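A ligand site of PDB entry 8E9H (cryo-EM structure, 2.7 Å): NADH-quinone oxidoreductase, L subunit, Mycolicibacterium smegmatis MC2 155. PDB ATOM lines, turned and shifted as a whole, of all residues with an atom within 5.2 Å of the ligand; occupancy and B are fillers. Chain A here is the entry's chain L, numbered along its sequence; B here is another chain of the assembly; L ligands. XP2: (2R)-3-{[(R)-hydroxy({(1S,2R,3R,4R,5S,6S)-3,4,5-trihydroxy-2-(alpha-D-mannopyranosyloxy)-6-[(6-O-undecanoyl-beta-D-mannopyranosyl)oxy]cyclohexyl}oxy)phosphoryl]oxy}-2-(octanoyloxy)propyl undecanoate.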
ATOM      1  N   PRO A 166      26.109   2.436  23.819  1.00  0.00           N
ATOM      2  CA  PRO A 166      25.898   3.896  23.790  1.00  0.00           C
ATOM      3  C   PRO A 166      26.083   4.549  25.141  1.00  0.00           C
ATOM      4  O   PRO A 166      26.523   5.707  25.208  1.00  0.00           O
ATOM      5  CB  PRO A 166      24.459   4.030  23.282  1.00  0.00           C
ATOM      6  CG  PRO A 166      24.180   2.764  22.563  1.00  0.00           C
ATOM      7  CD  PRO A 166      24.927   1.708  23.305  1.00  0.00           C
ATOM      8  N   SER A 167      25.735   3.862  26.225  1.00  0.00           N
ATOM      9  CA  SER A 167      25.884   4.454  27.555  1.00  0.00           C
ATOM     10  C   SER A 167      27.342   4.799  27.840  1.00  0.00           C
ATOM     11  O   SER A 167      27.628   5.857  28.418  1.00  0.00           O
ATOM     12  CB  SER A 167      25.343   3.494  28.611  1.00  0.00           C
ATOM     13  OG  SER A 167      25.999   2.245  28.535  1.00  0.00           O
ATOM     14  N   ALA A 168      28.262   3.933  27.443  1.00  0.00           N
ATOM     15  CA  ALA A 168      29.677   4.217  27.661  1.00  0.00           C
ATOM     16  C   ALA A 168      30.111   5.460  26.906  1.00  0.00           C
ATOM     17  O   ALA A 168      30.816   6.317  27.456  1.00  0.00           O
ATOM     18  CB  ALA A 168      30.530   3.012  27.245  1.00  0.00           C
ATOM     19  N   THR A 170      28.232   7.985  25.878  1.00  0.00           N
ATOM     20  CA  THR A 170      27.618   9.164  26.489  1.00  0.00           C
ATOM     21  C   THR A 170      28.330   9.534  27.780  1.00  0.00           C
ATOM     22  O   THR A 170      28.561  10.711  28.056  1.00  0.00           O
ATOM     23  CB  THR A 170      26.136   8.904  26.763  1.00  0.00           C
ATOM     24  OG1 THR A 170      25.506   8.479  25.553  1.00  0.00           O
ATOM     25  CG2 THR A 170      25.464  10.165  27.268  1.00  0.00           C
ATOM     26  N   LYS A 173      31.614  11.230  26.914  1.00  0.00           N
ATOM     27  CA  LYS A 173      31.383  12.591  26.469  1.00  0.00           C
ATOM     28  C   LYS A 173      31.083  13.506  27.645  1.00  0.00           C
ATOM     29  O   LYS A 173      31.633  14.607  27.747  1.00  0.00           O
ATOM     30  CB  LYS A 173      30.241  12.635  25.451  1.00  0.00           C
ATOM     31  CG  LYS A 173      29.992  14.019  24.861  1.00  0.00           C
ATOM     32  CD  LYS A 173      28.614  14.140  24.243  1.00  0.00           C
ATOM     33  CE  LYS A 173      27.521  14.021  25.282  1.00  0.00           C
ATOM     34  NZ  LYS A 173      26.214  14.555  24.806  1.00  0.00           N
ATOM     35  N   LYS A 174      30.192  13.078  28.534  1.00  0.00           N
ATOM     36  CA  LYS A 174      29.861  13.903  29.693  1.00  0.00           C
ATOM     37  C   LYS A 174      31.085  14.146  30.560  1.00  0.00           C
ATOM     38  O   LYS A 174      31.317  15.266  31.025  1.00  0.00           O
ATOM     39  CB  LYS A 174      28.765  13.237  30.518  1.00  0.00           C
ATOM     40  CG  LYS A 174      28.534  13.903  31.865  1.00  0.00           C
ATOM     41  CD  LYS A 174      27.148  13.650  32.408  1.00  0.00           C
ATOM     42  CE  LYS A 174      26.841  12.166  32.540  1.00  0.00           C
ATOM     43  NZ  LYS A 174      25.418  11.921  32.899  1.00  0.00           N
ATOM     44  N   VAL A 177      33.335  16.655  28.886  1.00  0.00           N
ATOM     45  CA  VAL A 177      32.765  18.000  28.840  1.00  0.00           C
ATOM     46  C   VAL A 177      32.881  18.673  30.208  1.00  0.00           C
ATOM     47  O   VAL A 177      33.270  19.838  30.326  1.00  0.00           O
ATOM     48  CB  VAL A 177      31.307  17.959  28.355  1.00  0.00           C
ATOM     49  CG1 VAL A 177      30.649  19.311  28.551  1.00  0.00           C
ATOM     50  CG2 VAL A 177      31.256  17.557  26.896  1.00  0.00           C
ATOM     51  N   VAL A 178      32.527  17.940  31.264  1.00  0.00           N
ATOM     52  CA  VAL A 178      32.618  18.516  32.609  1.00  0.00           C
ATOM     53  C   VAL A 178      34.064  18.802  32.954  1.00  0.00           C
ATOM     54  O   VAL A 178      34.402  19.881  33.486  1.00  0.00           O
ATOM     55  CB  VAL A 178      31.955  17.584  33.634  1.00  0.00           C
ATOM     56  CG1 VAL A 178      32.059  18.182  35.024  1.00  0.00           C
ATOM     57  CG2 VAL A 178      30.503  17.337  33.274  1.00  0.00           C
ATOM     58  N   VAL A 181      35.092  21.898  31.328  1.00  0.00           N
ATOM     59  CA  VAL A 181      34.665  23.086  32.053  1.00  0.00           C
ATOM     60  C   VAL A 181      35.651  23.377  33.179  1.00  0.00           C
ATOM     61  O   VAL A 181      36.070  24.533  33.399  1.00  0.00           O
ATOM     62  CB  VAL A 181      33.240  22.904  32.600  1.00  0.00           C
ATOM     63  CG1 VAL A 181      32.880  24.053  33.520  1.00  0.00           C
ATOM     64  CG2 VAL A 181      32.256  22.816  31.456  1.00  0.00           C
ATOM     65  N   MET A 184      38.649  24.778  31.660  1.00  0.00           N
ATOM     66  CA  MET A 184      38.427  26.179  31.328  1.00  0.00           C
ATOM     67  C   MET A 184      38.669  27.060  32.537  1.00  0.00           C
ATOM     68  O   MET A 184      39.325  28.105  32.439  1.00  0.00           O
ATOM     69  CB  MET A 184      37.000  26.364  30.808  1.00  0.00           C
ATOM     70  CG  MET A 184      36.678  27.779  30.389  1.00  0.00           C
ATOM     71  SD  MET A 184      34.995  27.934  29.765  1.00  0.00           S
ATOM     72  CE  MET A 184      34.065  27.774  31.278  1.00  0.00           C
ATOM     73  N   LEU A 226      37.472  25.630  40.786  1.00  0.00           N
ATOM     74  CA  LEU A 226      36.590  25.155  39.729  1.00  0.00           C
ATOM     75  C   LEU A 226      37.247  24.040  38.934  1.00  0.00           C
ATOM     76  O   LEU A 226      36.613  23.024  38.619  1.00  0.00           O
ATOM     77  CB  LEU A 226      36.211  26.320  38.809  1.00  0.00           C
ATOM     78  CG  LEU A 226      35.311  25.966  37.622  1.00  0.00           C
ATOM     79  CD1 LEU A 226      34.007  25.357  38.096  1.00  0.00           C
ATOM     80  CD2 LEU A 226      35.055  27.197  36.773  1.00  0.00           C
ATOM     81  N   PRO A 236      29.770  21.910  41.409  1.00  0.00           N
ATOM     82  CA  PRO A 236      28.643  21.411  40.616  1.00  0.00           C
ATOM     83  C   PRO A 236      29.066  20.464  39.495  1.00  0.00           C
ATOM     84  O   PRO A 236      28.223  20.040  38.705  1.00  0.00           O
ATOM     85  CB  PRO A 236      28.046  22.696  40.041  1.00  0.00           C
ATOM     86  CG  PRO A 236      29.236  23.565  39.832  1.00  0.00           C
ATOM     87  CD  PRO A 236      30.192  23.242  40.954  1.00  0.00           C
ATOM     88  N   SER A 239      28.486  15.433  38.576  1.00  0.00           N
ATOM     89  CA  SER A 239      27.520  14.521  37.985  1.00  0.00           C
ATOM     90  C   SER A 239      28.170  13.496  37.072  1.00  0.00           C
ATOM     91  O   SER A 239      27.554  12.462  36.778  1.00  0.00           O
ATOM     92  CB  SER A 239      26.476  15.314  37.207  1.00  0.00           C
ATOM     93  OG  SER A 239      27.081  16.177  36.263  1.00  0.00           O
ATOM     94  N   ASP A 553      21.884  15.456  37.776  1.00  0.00           N
ATOM     95  CA  ASP A 553      21.917  15.324  36.325  1.00  0.00           C
ATOM     96  C   ASP A 553      20.724  16.025  35.692  1.00  0.00           C
ATOM     97  O   ASP A 553      20.846  16.641  34.625  1.00  0.00           O
ATOM     98  CB  ASP A 553      21.947  13.846  35.933  1.00  0.00           C
ATOM     99  N   ASN A 556      21.465  19.691  35.299  1.00  0.00           N
ATOM    100  CA  ASN A 556      22.280  19.957  34.126  1.00  0.00           C
ATOM    101  C   ASN A 556      21.450  19.858  32.855  1.00  0.00           C
ATOM    102  O   ASN A 556      21.559  20.693  31.946  1.00  0.00           O
ATOM    103  CB  ASN A 556      23.459  18.986  34.061  1.00  0.00           C
ATOM    104  CG  ASN A 556      24.363  19.062  35.287  1.00  0.00           C
ATOM    105  OD1 ASN A 556      25.206  18.190  35.485  1.00  0.00           O
ATOM    106  ND2 ASN A 556      24.208  20.113  36.090  1.00  0.00           N
ATOM    107  N   GLU A 557      20.584  18.837  32.774  1.00  0.00           N
ATOM    108  CA  GLU A 557      19.766  18.660  31.593  1.00  0.00           C
ATOM    109  C   GLU A 557      18.833  19.830  31.372  1.00  0.00           C
ATOM    110  O   GLU A 557      18.640  20.275  30.233  1.00  0.00           O
ATOM    111  CB  GLU A 557      18.963  17.359  31.695  1.00  0.00           C
ATOM    112  CG  GLU A 557      19.822  16.103  31.692  1.00  0.00           C
ATOM    113  CD  GLU A 557      19.186  14.954  30.943  1.00  0.00           C
ATOM    114  OE1 GLU A 557      18.082  15.118  30.394  1.00  0.00           O
ATOM    115  OE2 GLU A 557      19.793  13.855  30.916  1.00  0.00           O
ATOM    116  N   PHE A 560      21.517  23.424  31.188  1.00  0.00           N
ATOM    117  CA  PHE A 560      22.552  23.514  30.162  1.00  0.00           C
ATOM    118  C   PHE A 560      22.184  22.772  28.894  1.00  0.00           C
ATOM    119  O   PHE A 560      22.281  23.342  27.800  1.00  0.00           O
ATOM    120  CB  PHE A 560      23.873  22.993  30.730  1.00  0.00           C
ATOM    121  CG  PHE A 560      24.414  23.835  31.850  1.00  0.00           C
ATOM    122  CD1 PHE A 560      25.172  24.961  31.589  1.00  0.00           C
ATOM    123  CD2 PHE A 560      24.126  23.512  33.163  1.00  0.00           C
ATOM    124  CE1 PHE A 560      25.664  25.725  32.619  1.00  0.00           C
ATOM    125  CE2 PHE A 560      24.612  24.282  34.198  1.00  0.00           C
ATOM    126  CZ  PHE A 560      25.382  25.395  33.927  1.00  0.00           C
ATOM    127  N   MET A 561      21.768  21.502  28.991  1.00  0.00           N
ATOM    128  CA  MET A 561      21.337  20.785  27.798  1.00  0.00           C
ATOM    129  C   MET A 561      20.144  21.481  27.152  1.00  0.00           C
ATOM    130  O   MET A 561      20.151  21.775  25.954  1.00  0.00           O
ATOM    131  CB  MET A 561      20.993  19.339  28.152  1.00  0.00           C
ATOM    132  CG  MET A 561      20.212  18.616  27.067  1.00  0.00           C
ATOM    133  SD  MET A 561      20.026  16.851  27.389  1.00  0.00           S
ATOM    134  CE  MET A 561      21.031  16.153  26.091  1.00  0.00           C
ATOM    135  N   GLY A 564      21.198  25.123  26.474  1.00  0.00           N
ATOM    136  CA  GLY A 564      22.150  25.075  25.374  1.00  0.00           C
ATOM    137  C   GLY A 564      21.478  24.791  24.042  1.00  0.00           C
ATOM    138  O   GLY A 564      21.815  25.410  23.030  1.00  0.00           O
ATOM    139  N   GLN A 565      20.533  23.854  24.021  1.00  0.00           N
ATOM    140  CA  GLN A 565      19.834  23.549  22.781  1.00  0.00           C
ATOM    141  C   GLN A 565      19.007  24.740  22.322  1.00  0.00           C
ATOM    142  O   GLN A 565      18.933  25.029  21.120  1.00  0.00           O
ATOM    143  CB  GLN A 565      18.941  22.327  22.975  1.00  0.00           C
ATOM    144  CG  GLN A 565      19.702  21.017  23.011  1.00  0.00           C
ATOM    145  CD  GLN A 565      18.812  19.841  23.324  1.00  0.00           C
ATOM    146  OE1 GLN A 565      17.719  19.999  23.869  1.00  0.00           O
ATOM    147  NE2 GLN A 565      19.274  18.641  22.997  1.00  0.00           N
ATOM    148  N   LEU A 567      19.701  27.914  22.887  1.00  0.00           N
ATOM    149  CA  LEU A 567      20.649  28.874  22.345  1.00  0.00           C
ATOM    150  C   LEU A 567      21.142  28.446  20.969  1.00  0.00           C
ATOM    151  O   LEU A 567      21.292  29.279  20.068  1.00  0.00           O
ATOM    152  CB  LEU A 567      21.827  29.045  23.309  1.00  0.00           C
ATOM    153  CG  LEU A 567      22.972  29.943  22.825  1.00  0.00           C
ATOM    154  CD1 LEU A 567      22.475  31.359  22.599  1.00  0.00           C
ATOM    155  CD2 LEU A 567      24.109  29.928  23.839  1.00  0.00           C
ATOM    156  N   THR A 568      21.409  27.152  20.796  1.00  0.00           N
ATOM    157  CA  THR A 568      21.874  26.652  19.517  1.00  0.00           C
ATOM    158  C   THR A 568      20.825  26.863  18.433  1.00  0.00           C
ATOM    159  O   THR A 568      21.140  27.284  17.316  1.00  0.00           O
ATOM    160  CB  THR A 568      22.236  25.176  19.632  1.00  0.00           C
ATOM    161  OG1 THR A 568      23.261  25.010  20.616  1.00  0.00           O
ATOM    162  CG2 THR A 568      22.740  24.649  18.294  1.00  0.00           C
ATOM    163  N   ILE B 315      27.869  23.092  16.843  1.00  0.00           N
ATOM    164  CA  ILE B 315      27.054  22.233  17.692  1.00  0.00           C
ATOM    165  C   ILE B 315      25.712  21.966  17.034  1.00  0.00           C
ATOM    166  O   ILE B 315      25.188  20.850  17.074  1.00  0.00           O
ATOM    167  CB  ILE B 315      26.875  22.840  19.091  1.00  0.00           C
ATOM    168  CG1 ILE B 315      28.228  22.998  19.799  1.00  0.00           C
ATOM    169  CG2 ILE B 315      25.967  21.964  19.918  1.00  0.00           C
ATOM    170  CD1 ILE B 315      28.170  23.881  21.028  1.00  0.00           C
ATOM    171  N   VAL B 439      35.196  24.803  26.012  1.00  0.00           N
ATOM    172  CA  VAL B 439      34.123  23.854  26.309  1.00  0.00           C
ATOM    173  C   VAL B 439      33.303  23.581  25.051  1.00  0.00           C
ATOM    174  O   VAL B 439      32.906  22.440  24.779  1.00  0.00           O
ATOM    175  CB  VAL B 439      33.240  24.381  27.450  1.00  0.00           C
ATOM    176  CG1 VAL B 439      32.127  23.402  27.760  1.00  0.00           C
ATOM    177  CG2 VAL B 439      34.078  24.657  28.683  1.00  0.00           C
ATOM    178  N   LEU B 440      33.018  24.628  24.281  1.00  0.00           N
ATOM    179  CA  LEU B 440      32.183  24.437  23.098  1.00  0.00           C
ATOM    180  C   LEU B 440      32.832  23.497  22.098  1.00  0.00           C
ATOM    181  O   LEU B 440      32.138  22.716  21.429  1.00  0.00           O
ATOM    182  CB  LEU B 440      31.868  25.781  22.449  1.00  0.00           C
ATOM    183  CG  LEU B 440      31.148  26.773  23.346  1.00  0.00           C
ATOM    184  CD1 LEU B 440      31.064  28.131  22.679  1.00  0.00           C
ATOM    185  CD2 LEU B 440      29.775  26.268  23.713  1.00  0.00           C
ATOM    186  N   VAL B 443      32.329  20.014  23.173  1.00  0.00           N
ATOM    187  CA  VAL B 443      30.969  19.618  22.846  1.00  0.00           C
ATOM    188  C   VAL B 443      30.877  19.204  21.378  1.00  0.00           C
ATOM    189  O   VAL B 443      30.554  18.064  21.051  1.00  0.00           O
ATOM    190  CB  VAL B 443      29.975  20.738  23.176  1.00  0.00           C
ATOM    191  CG1 VAL B 443      28.584  20.345  22.734  1.00  0.00           C
ATOM    192  CG2 VAL B 443      29.996  21.028  24.663  1.00  0.00           C
ATOM    193  N   TRP B 447      30.544  15.177  20.794  1.00  0.00           N
ATOM    194  CA  TRP B 447      29.183  14.766  20.465  1.00  0.00           C
ATOM    195  C   TRP B 447      29.102  14.207  19.052  1.00  0.00           C
ATOM    196  O   TRP B 447      28.441  13.193  18.821  1.00  0.00           O
ATOM    197  CB  TRP B 447      28.227  15.939  20.638  1.00  0.00           C
ATOM    198  CG  TRP B 447      26.805  15.572  20.399  1.00  0.00           C
ATOM    199  CD1 TRP B 447      26.230  14.355  20.585  1.00  0.00           C
ATOM    200  CD2 TRP B 447      25.761  16.438  19.934  1.00  0.00           C
ATOM    201  NE1 TRP B 447      24.891  14.399  20.276  1.00  0.00           N
ATOM    202  CE2 TRP B 447      24.580  15.668  19.876  1.00  0.00           C
ATOM    203  CE3 TRP B 447      25.700  17.784  19.574  1.00  0.00           C
ATOM    204  CZ2 TRP B 447      23.372  16.200  19.452  1.00  0.00           C
ATOM    205  CZ3 TRP B 447      24.497  18.315  19.159  1.00  0.00           C
ATOM    206  CH2 TRP B 447      23.345  17.522  19.101  1.00  0.00           C
ATOM    207  N   GLN B 450      30.639  10.788  19.144  1.00  0.00           N
ATOM    208  CA  GLN B 450      29.686   9.859  19.719  1.00  0.00           C
ATOM    209  C   GLN B 450      28.638   9.459  18.697  1.00  0.00           C
ATOM    210  O   GLN B 450      28.277   8.290  18.557  1.00  0.00           O
ATOM    211  CB  GLN B 450      29.037  10.483  20.955  1.00  0.00           C
ATOM    212  CG  GLN B 450      27.890   9.696  21.547  1.00  0.00           C
ATOM    213  CD  GLN B 450      27.164  10.470  22.612  1.00  0.00           C
ATOM    214  OE1 GLN B 450      27.768  11.233  23.359  1.00  0.00           O
ATOM    215  NE2 GLN B 450      25.853  10.280  22.697  1.00  0.00           N
HETATM  216  C02 XP2 L   1      19.849  10.613  26.511  1.00  0.00           C
HETATM  217  C03 XP2 L   1      19.286  12.008  26.833  1.00  0.00           C
HETATM  218  C05 XP2 L   1      20.182  12.730  27.870  1.00  0.00           C
HETATM  219  C07 XP2 L   1      21.635  12.616  27.468  1.00  0.00           C
HETATM  220  C09 XP2 L   1      22.460  14.114  28.950  1.00  0.00           C
HETATM  221  C11 XP2 L   1      22.816  15.899  30.550  1.00  0.00           C
HETATM  222  C12 XP2 L   1      23.503  17.226  30.752  1.00  0.00           C
HETATM  223  C14 XP2 L   1      25.842  17.504  30.248  1.00  0.00           C
HETATM  224  C15 XP2 L   1      26.051  17.464  31.768  1.00  0.00           C
HETATM  225  C16 XP2 L   1      27.205  18.392  32.198  1.00  0.00           C
HETATM  226  C17 XP2 L   1      26.998  19.823  31.710  1.00  0.00           C
HETATM  227  C18 XP2 L   1      28.213  20.697  32.023  1.00  0.00           C
HETATM  228  C19 XP2 L   1      27.836  21.870  32.972  1.00  0.00           C
HETATM  229  C20 XP2 L   1      27.415  21.336  34.362  1.00  0.00           C
HETATM  230  C21 XP2 L   1      27.242  22.504  35.423  1.00  0.00           C
HETATM  231  C22 XP2 L   1      28.435  23.499  35.371  1.00  0.00           C
HETATM  232  C23 XP2 L   1      28.238  24.694  36.354  1.00  0.00           C
HETATM  233  C24 XP2 L   1      29.490  25.603  36.432  1.00  0.00           C
HETATM  234  C26 XP2 L   1      23.494  14.820  31.401  1.00  0.00           C
HETATM  235  C28 XP2 L   1      24.320  13.897  30.550  1.00  0.00           C
HETATM  236  C30 XP2 L   1      23.494  13.177  29.549  1.00  0.00           C
HETATM  237  C32 XP2 L   1      21.717  12.192  26.007  1.00  0.00           C
HETATM  238  C36 XP2 L   1      23.447  15.660  23.321  1.00  0.00           C
HETATM  239  C37 XP2 L   1      23.476  17.078  23.910  1.00  0.00           C
HETATM  240  C39 XP2 L   1      23.637  19.161  22.882  1.00  0.00           C
HETATM  241  C40 XP2 L   1      24.422  20.495  23.125  1.00  0.00           C
HETATM  242  C41 XP2 L   1      23.529  21.701  22.806  1.00  0.00           C
HETATM  243  C42 XP2 L   1      24.225  23.070  23.195  1.00  0.00           C
HETATM  244  C43 XP2 L   1      25.406  22.849  24.243  1.00  0.00           C
HETATM  245  C44 XP2 L   1      26.208  24.172  24.458  1.00  0.00           C
HETATM  246  C45 XP2 L   1      26.150  24.660  25.924  1.00  0.00           C
HETATM  247  C46 XP2 L   1      26.560  26.144  26.055  1.00  0.00           C
HETATM  248  C48 XP2 L   1      24.053  17.015  25.318  1.00  0.00           C
HETATM  249  C50 XP2 L   1      25.809  18.191  26.397  1.00  0.00           C
HETATM  250  C51 XP2 L   1      24.801  19.206  26.996  1.00  0.00           C
HETATM  251  C52 XP2 L   1      25.520  20.245  27.892  1.00  0.00           C
HETATM  252  C53 XP2 L   1      26.549  21.097  27.072  1.00  0.00           C
HETATM  253  C54 XP2 L   1      27.695  21.628  27.981  1.00  0.00           C
HETATM  254  C55 XP2 L   1      27.190  22.748  28.916  1.00  0.00           C
HETATM  255  C56 XP2 L   1      28.335  23.457  29.642  1.00  0.00           C
HETATM  256  C57 XP2 L   1      28.093  25.005  29.739  1.00  0.00           C
HETATM  257  C58 XP2 L   1      28.966  25.652  30.844  1.00  0.00           C
HETATM  258  C59 XP2 L   1      29.693  26.981  30.338  1.00  0.00           C
HETATM  259  C60 XP2 L   1      30.299  27.812  31.521  1.00  0.00           C
HETATM  260  C64 XP2 L   1      21.232  10.734  25.898  1.00  0.00           C
HETATM  261  C66 XP2 L   1      22.348   9.591  24.232  1.00  0.00           C
HETATM  262  C67 XP2 L   1      21.968   8.649  23.103  1.00  0.00           C
HETATM  263  C69 XP2 L   1      21.047   7.582  23.594  1.00  0.00           C
HETATM  264  C71 XP2 L   1      21.720   6.804  24.624  1.00  0.00           C
HETATM  265  C73 XP2 L   1      22.043   7.681  25.810  1.00  0.00           C
HETATM  266  C74 XP2 L   1      22.836   6.905  26.776  1.00  0.00           C
HETATM  267  O01 XP2 L   1      18.997   9.964  25.604  1.00  0.00           O
HETATM  268  O04 XP2 L   1      18.011  11.877  27.364  1.00  0.00           O
HETATM  269  O06 XP2 L   1      19.792  14.075  27.904  1.00  0.00           O
HETATM  270  O08 XP2 L   1      22.350  13.883  27.639  1.00  0.00           O
HETATM  271  O10 XP2 L   1      22.859  15.556  29.120  1.00  0.00           O
HETATM  272  O13 XP2 L   1      24.515  17.368  29.713  1.00  0.00           O
HETATM  273  O25 XP2 L   1      26.772  17.634  29.519  1.00  0.00           O
HETATM  274  O27 XP2 L   1      22.487  14.049  32.068  1.00  0.00           O
HETATM  275  O29 XP2 L   1      25.287  14.706  29.832  1.00  0.00           O
HETATM  276  O31 XP2 L   1      24.373  12.688  28.529  1.00  0.00           O
HETATM  277  O33 XP2 L   1      23.061  12.269  25.541  1.00  0.00           O
HETATM  278  O35 XP2 L   1      23.346  14.757  24.438  1.00  0.00           O
HETATM  279  O38 XP2 L   1      24.257  17.893  23.117  1.00  0.00           O
HETATM  280  O47 XP2 L   1      22.528  19.213  22.506  1.00  0.00           O
HETATM  281  O49 XP2 L   1      25.436  17.391  25.274  1.00  0.00           O
HETATM  282  O61 XP2 L   1      26.890  18.091  26.862  1.00  0.00           O
HETATM  283  O62 XP2 L   1      22.219  12.826  23.144  1.00  0.00           O
HETATM  284  O63 XP2 L   1      24.621  12.708  23.520  1.00  0.00           O
HETATM  285  O65 XP2 L   1      21.189  10.358  24.551  1.00  0.00           O
HETATM  286  O68 XP2 L   1      23.149   8.045  22.607  1.00  0.00           O
HETATM  287  O70 XP2 L   1      20.662   6.706  22.492  1.00  0.00           O
HETATM  288  O72 XP2 L   1      20.862   5.736  25.069  1.00  0.00           O
HETATM  289  O75 XP2 L   1      23.898   6.288  26.053  1.00  0.00           O
HETATM  290  O76 XP2 L   1      22.840   8.907  25.411  1.00  0.00           O
HETATM  291  P34 XP2 L   1      23.324  13.119  24.108  1.00  0.00           P
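OD1 of Asn 556 lies within hydrogen-bond range of OG of Ser 239 (2.9 Å). The side-chain hydroxyl (OG1) of Thr 568 sits at hydrogen-bond distance from the backbone carbonyl oxygen (O) of Gly 564, 2.8 Å away. O of Asn 556 is in hydrogen-bond range of N of Met 561 (3.1 Å). The side-chain hydroxyl of Thr 170 is in hydrogen-bond range of the side-chain amide nitrogen of Gln 450 of chain B (3.4 Å). O of Pro 166 sits at hydrogen-bond distance from OG1 of Thr 170 (3.0 Å).
O63 of the ligand is in hydrogen-bond range of NE2 of Gln 450 of chain B, at 2.8 Å. The side-chain sulfur of Met 561 sits at hydrogen-bond distance from an oxygen (O06) of the ligand. N of Ser 167 sits at hydrogen-bond distance from O75 of the ligand (3.0 Å). The side-chain amide nitrogen of Gln 565 is in hydrogen-bond range of an oxygen (O47) of the ligand (3.3 Å). The side-chain carboxylate of Glu 557 is in hydrogen-bond range of an oxygen (O27) of the ligand (2.9 Å). The side-chain amino group of Lys 173 is in salt-bridge range of an oxygen (O63) of the ligand (2.8 Å). An oxygen (O76) of the ligand lies within hydrogen-bond range of the side-chain hydroxyl of Thr 170 (2.7 Å). The backbone carbonyl oxygen (O) of Pro 166 is in hydrogen-bond range of an oxygen (O75) of the ligand (2.8 Å).
NZ of Lys 174 touches C28 of the ligand, at 3.3 Å. Val 177 touches the ligand (CG1 to C54, 3.8 Å). Val 178 touches the ligand (CG2 to C16, 3.6 Å). CE of Met 184 touches C60 of the ligand (3.8 Å). Pro 236 touches the ligand. CB of Asp 553 touches O27 of the ligand, 3.9 Å away. Asn 556 touches the ligand. CE2 of Phe 560 touches C21 of the ligand, 3.4 Å away. Gly 564 touches the ligand (C to C42, 3.4 Å). OG1 of Thr 568 touches C42 of the ligand, at 3.4 Å. Ile 315 of chain B touches the ligand (CG2 to C41, 3.8 Å). Leu 440 of chain B touches the ligand (CD2 to C46, 3.98 Å). NE1 of Trp 447 of chain B touches C36 of the ligand, 3.6 Å away. Hydrophobic or aromatic side chains within 4 Å of the ligand: Pro 166, Val 177, Val 178, Met 184, Pro 236, Phe 560, Met 561, Ile 315 of chain B, Leu 440 of chain B and Trp 447 of chain B. Within 4 Å of the ligand: Pro 166, Ser 167, Thr 170, Lys 173, Lys 174, Val 177, Val 178, Met 184, Pro 236, Asp 553, Asn 556, Glu 557, Phe 560, Met 561, Gly 564, Gln 565, Thr 568, Ile 315 of chain B, Leu 440 of chain B, Trp 447 of chain B and Gln 450 of chain B.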
